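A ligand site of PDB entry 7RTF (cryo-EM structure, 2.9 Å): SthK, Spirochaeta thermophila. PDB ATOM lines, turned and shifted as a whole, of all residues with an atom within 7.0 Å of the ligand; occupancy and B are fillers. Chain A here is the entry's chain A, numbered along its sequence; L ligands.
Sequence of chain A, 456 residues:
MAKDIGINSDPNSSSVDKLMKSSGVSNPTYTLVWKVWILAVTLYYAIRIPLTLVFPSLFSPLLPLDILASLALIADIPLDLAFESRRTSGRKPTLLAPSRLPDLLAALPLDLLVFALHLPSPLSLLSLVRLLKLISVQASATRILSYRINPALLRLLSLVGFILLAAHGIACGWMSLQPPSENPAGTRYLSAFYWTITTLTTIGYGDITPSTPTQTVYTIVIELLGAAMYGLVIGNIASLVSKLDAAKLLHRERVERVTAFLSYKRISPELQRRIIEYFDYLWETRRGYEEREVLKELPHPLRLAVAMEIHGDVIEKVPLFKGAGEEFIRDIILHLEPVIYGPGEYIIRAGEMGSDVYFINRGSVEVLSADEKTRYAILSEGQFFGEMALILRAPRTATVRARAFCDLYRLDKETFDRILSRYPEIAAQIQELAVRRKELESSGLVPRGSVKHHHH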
ATOM      1  N   ILE A 348      23.234  26.255  21.192  1.00  0.00           N
ATOM      2  CA  ILE A 348      22.539  25.217  20.426  1.00  0.00           C
ATOM      3  C   ILE A 348      23.492  24.042  20.241  1.00  0.00           C
ATOM      4  O   ILE A 348      24.648  24.241  19.858  1.00  0.00           O
ATOM      5  CB  ILE A 348      22.041  25.759  19.071  1.00  0.00           C
ATOM      6  CG1 ILE A 348      20.808  26.630  19.265  1.00  0.00           C
ATOM      7  CG2 ILE A 348      21.731  24.621  18.103  1.00  0.00           C
ATOM      8  CD1 ILE A 348      20.381  27.377  18.024  1.00  0.00           C
ATOM      9  N   MET A 353      16.527  18.414  19.014  1.00  0.00           N
ATOM     10  CA  MET A 353      15.300  18.869  18.376  1.00  0.00           C
ATOM     11  C   MET A 353      15.233  20.393  18.286  1.00  0.00           C
ATOM     12  O   MET A 353      15.290  20.957  17.184  1.00  0.00           O
ATOM     13  CB  MET A 353      14.086  18.332  19.138  1.00  0.00           C
ATOM     14  CG  MET A 353      13.840  16.854  18.920  1.00  0.00           C
ATOM     15  SD  MET A 353      13.670  16.424  17.176  1.00  0.00           S
ATOM     16  CE  MET A 353      15.058  15.319  16.971  1.00  0.00           C
ATOM     17  N   ASP A 356      13.342  27.019  19.490  1.00  0.00           N
ATOM     18  CA  ASP A 356      13.423  28.452  19.741  1.00  0.00           C
ATOM     19  C   ASP A 356      14.072  29.176  18.563  1.00  0.00           C
ATOM     20  O   ASP A 356      14.614  28.565  17.644  1.00  0.00           O
ATOM     21  CB  ASP A 356      14.188  28.728  21.033  1.00  0.00           C
ATOM     22  CG  ASP A 356      13.444  28.276  22.267  1.00  0.00           C
ATOM     23  OD1 ASP A 356      13.384  29.046  23.250  1.00  0.00           O
ATOM     24  OD2 ASP A 356      12.910  27.148  22.253  1.00  0.00           O
ATOM     25  N   VAL A 367      29.412  30.103  14.597  1.00  0.00           N
ATOM     26  CA  VAL A 367      28.725  28.883  14.166  1.00  0.00           C
ATOM     27  C   VAL A 367      29.747  27.828  13.774  1.00  0.00           C
ATOM     28  O   VAL A 367      30.585  28.047  12.885  1.00  0.00           O
ATOM     29  CB  VAL A 367      27.761  29.173  13.002  1.00  0.00           C
ATOM     30  CG1 VAL A 367      27.193  27.866  12.460  1.00  0.00           C
ATOM     31  CG2 VAL A 367      26.653  30.104  13.456  1.00  0.00           C
ATOM     32  N   TYR A 376      31.769  27.834  10.399  1.00  0.00           N
ATOM     33  CA  TYR A 376      30.982  28.238   9.239  1.00  0.00           C
ATOM     34  C   TYR A 376      30.973  29.754   9.092  1.00  0.00           C
ATOM     35  O   TYR A 376      31.463  30.297   8.093  1.00  0.00           O
ATOM     36  CB  TYR A 376      29.556  27.694   9.370  1.00  0.00           C
ATOM     37  CG  TYR A 376      29.431  26.186   9.213  1.00  0.00           C
ATOM     38  CD1 TYR A 376      30.516  25.415   8.799  1.00  0.00           C
ATOM     39  CD2 TYR A 376      28.232  25.539   9.484  1.00  0.00           C
ATOM     40  CE1 TYR A 376      30.401  24.040   8.665  1.00  0.00           C
ATOM     41  CE2 TYR A 376      28.115  24.172   9.345  1.00  0.00           C
ATOM     42  CZ  TYR A 376      29.196  23.430   8.938  1.00  0.00           C
ATOM     43  OH  TYR A 376      29.079  22.063   8.798  1.00  0.00           O
ATOM     44  N   ALA A 377      30.436  30.469  10.084  1.00  0.00           N
ATOM     45  CA  ALA A 377      30.280  31.909   9.971  1.00  0.00           C
ATOM     46  C   ALA A 377      30.271  32.537  11.361  1.00  0.00           C
ATOM     47  O   ALA A 377      30.313  31.837  12.386  1.00  0.00           O
ATOM     48  CB  ALA A 377      29.008  32.256   9.201  1.00  0.00           C
ATOM     49  N   ILE A 378      30.218  33.866  11.385  1.00  0.00           N
ATOM     50  CA  ILE A 378      30.186  34.634  12.624  1.00  0.00           C
ATOM     51  C   ILE A 378      29.052  35.638  12.525  1.00  0.00           C
ATOM     52  O   ILE A 378      28.991  36.424  11.579  1.00  0.00           O
ATOM     53  CB  ILE A 378      31.522  35.363  12.873  1.00  0.00           C
ATOM     54  CG1 ILE A 378      32.617  34.354  13.236  1.00  0.00           C
ATOM     55  CG2 ILE A 378      31.376  36.416  13.959  1.00  0.00           C
ATOM     56  CD1 ILE A 378      33.976  34.980  13.436  1.00  0.00           C
ATOM     57  N   LEU A 379      28.141  35.607  13.500  1.00  0.00           N
ATOM     58  CA  LEU A 379      27.034  36.541  13.561  1.00  0.00           C
ATOM     59  C   LEU A 379      27.276  37.585  14.645  1.00  0.00           C
ATOM     60  O   LEU A 379      27.895  37.303  15.678  1.00  0.00           O
ATOM     61  CB  LEU A 379      25.720  35.800  13.826  1.00  0.00           C
ATOM     62  CG  LEU A 379      25.527  34.480  13.085  1.00  0.00           C
ATOM     63  CD1 LEU A 379      24.229  33.802  13.486  1.00  0.00           C
ATOM     64  CD2 LEU A 379      25.582  34.704  11.587  1.00  0.00           C
ATOM     65  N   PHE A 384      20.302  37.110  13.379  1.00  0.00           N
ATOM     66  CA  PHE A 384      19.535  36.103  14.104  1.00  0.00           C
ATOM     67  C   PHE A 384      19.885  34.716  13.583  1.00  0.00           C
ATOM     68  O   PHE A 384      20.410  34.561  12.474  1.00  0.00           O
ATOM     69  CB  PHE A 384      18.030  36.353  13.977  1.00  0.00           C
ATOM     70  CG  PHE A 384      17.506  36.277  12.567  1.00  0.00           C
ATOM     71  CD1 PHE A 384      17.642  37.355  11.707  1.00  0.00           C
ATOM     72  CD2 PHE A 384      16.890  35.133  12.099  1.00  0.00           C
ATOM     73  CE1 PHE A 384      17.175  37.293  10.415  1.00  0.00           C
ATOM     74  CE2 PHE A 384      16.418  35.064  10.801  1.00  0.00           C
ATOM     75  CZ  PHE A 384      16.559  36.148   9.964  1.00  0.00           C
ATOM     76  N   PHE A 385      19.596  33.709  14.401  1.00  0.00           N
ATOM     77  CA  PHE A 385      19.852  32.317  14.027  1.00  0.00           C
ATOM     78  C   PHE A 385      18.756  31.458  14.634  1.00  0.00           C
ATOM     79  O   PHE A 385      18.033  31.864  15.545  1.00  0.00           O
ATOM     80  CB  PHE A 385      21.236  31.843  14.489  1.00  0.00           C
ATOM     81  CG  PHE A 385      21.524  32.108  15.941  1.00  0.00           C
ATOM     82  CD1 PHE A 385      21.178  31.176  16.911  1.00  0.00           C
ATOM     83  CD2 PHE A 385      22.157  33.274  16.340  1.00  0.00           C
ATOM     84  CE1 PHE A 385      21.454  31.406  18.246  1.00  0.00           C
ATOM     85  CE2 PHE A 385      22.429  33.512  17.669  1.00  0.00           C
ATOM     86  CZ  PHE A 385      22.076  32.581  18.628  1.00  0.00           C
ATOM     87  N   GLY A 386      18.638  30.238  14.107  1.00  0.00           N
ATOM     88  CA  GLY A 386      17.639  29.310  14.604  1.00  0.00           C
ATOM     89  C   GLY A 386      16.245  29.475  14.031  1.00  0.00           C
ATOM     90  O   GLY A 386      15.297  28.916  14.596  1.00  0.00           O
ATOM     91  N   GLU A 387      16.087  30.213  12.935  1.00  0.00           N
ATOM     92  CA  GLU A 387      14.768  30.458  12.367  1.00  0.00           C
ATOM     93  C   GLU A 387      14.123  29.202  11.790  1.00  0.00           C
ATOM     94  O   GLU A 387      12.916  29.213  11.522  1.00  0.00           O
ATOM     95  CB  GLU A 387      14.847  31.535  11.280  1.00  0.00           C
ATOM     96  CG  GLU A 387      15.532  31.087  10.003  1.00  0.00           C
ATOM     97  CD  GLU A 387      16.996  31.477   9.959  1.00  0.00           C
ATOM     98  OE1 GLU A 387      17.394  32.163   8.991  1.00  0.00           O
ATOM     99  OE2 GLU A 387      17.740  31.113  10.888  1.00  0.00           O
ATOM    100  N   MET A 388      14.897  28.122  11.611  1.00  0.00           N
ATOM    101  CA  MET A 388      14.353  26.898  11.032  1.00  0.00           C
ATOM    102  C   MET A 388      13.491  26.118  12.018  1.00  0.00           C
ATOM    103  O   MET A 388      12.706  25.267  11.581  1.00  0.00           O
ATOM    104  CB  MET A 388      15.488  26.000  10.539  1.00  0.00           C
ATOM    105  CG  MET A 388      15.764  26.092   9.053  1.00  0.00           C
ATOM    106  SD  MET A 388      17.293  25.246   8.608  1.00  0.00           S
ATOM    107  CE  MET A 388      18.292  26.629   8.072  1.00  0.00           C
ATOM    108  N   ALA A 389      13.612  26.384  13.315  1.00  0.00           N
ATOM    109  CA  ALA A 389      12.859  25.614  14.299  1.00  0.00           C
ATOM    110  C   ALA A 389      11.388  26.002  14.316  1.00  0.00           C
ATOM    111  O   ALA A 389      10.542  25.169  14.676  1.00  0.00           O
ATOM    112  CB  ALA A 389      13.470  25.805  15.687  1.00  0.00           C
ATOM    113  N   ALA A 394      12.384  19.793  13.002  1.00  0.00           N
ATOM    114  CA  ALA A 394      13.539  19.041  12.545  1.00  0.00           C
ATOM    115  C   ALA A 394      14.718  19.277  13.487  1.00  0.00           C
ATOM    116  O   ALA A 394      14.817  20.329  14.128  1.00  0.00           O
ATOM    117  CB  ALA A 394      13.909  19.465  11.127  1.00  0.00           C
ATOM    118  N   PRO A 395      15.635  18.310  13.599  1.00  0.00           N
ATOM    119  CA  PRO A 395      16.806  18.494  14.452  1.00  0.00           C
ATOM    120  C   PRO A 395      17.714  19.589  13.931  1.00  0.00           C
ATOM    121  O   PRO A 395      17.721  19.908  12.736  1.00  0.00           O
ATOM    122  CB  PRO A 395      17.499  17.126  14.426  1.00  0.00           C
ATOM    123  CG  PRO A 395      16.983  16.474  13.184  1.00  0.00           C
ATOM    124  CD  PRO A 395      15.585  16.951  13.022  1.00  0.00           C
ATOM    125  N   ARG A 396      18.475  20.185  14.848  1.00  0.00           N
ATOM    126  CA  ARG A 396      19.386  21.272  14.512  1.00  0.00           C
ATOM    127  C   ARG A 396      20.435  20.807  13.503  1.00  0.00           C
ATOM    128  O   ARG A 396      20.643  19.612  13.269  1.00  0.00           O
ATOM    129  CB  ARG A 396      20.069  21.816  15.772  1.00  0.00           C
ATOM    130  CG  ARG A 396      19.108  22.255  16.863  1.00  0.00           C
ATOM    131  CD  ARG A 396      18.336  23.497  16.460  1.00  0.00           C
ATOM    132  NE  ARG A 396      17.826  24.222  17.615  1.00  0.00           N
ATOM    133  CZ  ARG A 396      17.191  25.383  17.553  1.00  0.00           C
ATOM    134  NH1 ARG A 396      16.959  25.978  16.398  1.00  0.00           N
ATOM    135  NH2 ARG A 396      16.770  25.950  18.675  1.00  0.00           N
ATOM    136  N   THR A 397      21.115  21.774  12.890  1.00  0.00           N
ATOM    137  CA  THR A 397      22.061  21.516  11.829  1.00  0.00           C
ATOM    138  C   THR A 397      23.469  22.023  12.106  1.00  0.00           C
ATOM    139  O   THR A 397      24.394  21.638  11.381  1.00  0.00           O
ATOM    140  CB  THR A 397      21.579  22.133  10.501  1.00  0.00           C
ATOM    141  OG1 THR A 397      21.559  23.567  10.622  1.00  0.00           O
ATOM    142  CG2 THR A 397      20.184  21.642  10.149  1.00  0.00           C
ATOM    143  N   ALA A 398      23.663  22.855  13.128  1.00  0.00           N
ATOM    144  CA  ALA A 398      24.990  23.330  13.471  1.00  0.00           C
ATOM    145  C   ALA A 398      25.015  23.777  14.929  1.00  0.00           C
ATOM    146  O   ALA A 398      23.967  24.015  15.542  1.00  0.00           O
ATOM    147  CB  ALA A 398      25.434  24.480  12.564  1.00  0.00           C
ATOM    148  N   THR A 399      26.223  23.875  15.462  1.00  0.00           N
ATOM    149  CA  THR A 399      26.470  24.237  16.853  1.00  0.00           C
ATOM    150  C   THR A 399      26.723  25.734  16.915  1.00  0.00           C
ATOM    151  O   THR A 399      27.283  26.327  15.989  1.00  0.00           O
ATOM    152  CB  THR A 399      27.666  23.425  17.395  1.00  0.00           C
ATOM    153  OG1 THR A 399      27.243  22.085  17.658  1.00  0.00           O
ATOM    154  CG2 THR A 399      28.243  24.007  18.688  1.00  0.00           C
ATOM    155  N   VAL A 400      26.308  26.352  18.016  1.00  0.00           N
ATOM    156  CA  VAL A 400      26.356  27.801  18.181  1.00  0.00           C
ATOM    157  C   VAL A 400      27.047  28.111  19.500  1.00  0.00           C
ATOM    158  O   VAL A 400      26.613  27.656  20.563  1.00  0.00           O
ATOM    159  CB  VAL A 400      24.949  28.410  18.157  1.00  0.00           C
ATOM    160  CG1 VAL A 400      24.959  29.821  18.683  1.00  0.00           C
ATOM    161  CG2 VAL A 400      24.381  28.371  16.748  1.00  0.00           C
HETATM  162  P1  LIG L   1      18.745  25.490  13.084  1.00  0.00           P
HETATM  163  O1  LIG L   1      17.854  24.436  12.462  1.00  0.00           O
HETATM  164  O2  LIG L   1      18.339  26.118  14.393  1.00  0.00           O
HETATM  165  O3  LIG L   1      20.190  24.837  13.314  1.00  0.00           O
HETATM  166  C1  LIG L   1      21.301  25.648  13.700  1.00  0.00           C
HETATM  167  C2  LIG L   1      21.159  26.988  13.040  1.00  0.00           C
HETATM  168  O4  LIG L   1      22.417  27.552  12.622  1.00  0.00           O
HETATM  169  C3  LIG L   1      20.368  26.945  11.769  1.00  0.00           C
HETATM  170  O5  LIG L   1      19.003  26.673  12.006  1.00  0.00           O
HETATM  171  C4  LIG L   1      20.707  28.287  11.134  1.00  0.00           C
HETATM  172  O6  LIG L   1      19.989  29.330  11.758  1.00  0.00           O
HETATM  173  C5  LIG L   1      22.194  28.423  11.531  1.00  0.00           C
HETATM  174  N1  LIG L   1      23.100  28.030  10.423  1.00  0.00           N
HETATM  175  C6  LIG L   1      23.232  26.811   9.885  1.00  0.00           C
HETATM  176  N2  LIG L   1      24.157  26.805   8.886  1.00  0.00           N
HETATM  177  C7  LIG L   1      24.626  28.065   8.776  1.00  0.00           C
HETATM  178  C8  LIG L   1      25.622  28.752   7.917  1.00  0.00           C
HETATM  179  N3  LIG L   1      26.305  28.088   6.966  1.00  0.00           N
HETATM  180  N4  LIG L   1      25.822  30.072   8.132  1.00  0.00           N
HETATM  181  C9  LIG L   1      25.144  30.742   9.073  1.00  0.00           C
HETATM  182  N5  LIG L   1      24.232  30.180   9.887  1.00  0.00           N
HETATM  183  C10 LIG L   1      23.928  28.865   9.785  1.00  0.00           C
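N of Gly 386 is in hydrogen-bond range of O6 of the ligand (2.9 Å).
The backbone NH of Thr 397 lies within hydrogen-bond range of an oxygen (O3) of the ligand, 3.2 Å away.
The side-chain carboxylate of Glu 387 sits at hydrogen-bond distance from an oxygen (O6) of the ligand, at 3.0 Å.
O3 of the ligand sits at hydrogen-bond distance from OG1 of Thr 397, at 3.3 Å.
An oxygen (O2) of the ligand lies within salt-bridge range of the guanidinium group (NH1) of Arg 396 (2.4 Å).
Residues that only touch the ligand: Phe 385 (3.8 Å), Met 388 (3.4 Å) and Ala 398 (3.6 Å).
Hydrophobic or aromatic side chains that line the ligand: Phe 385 and Met 388.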
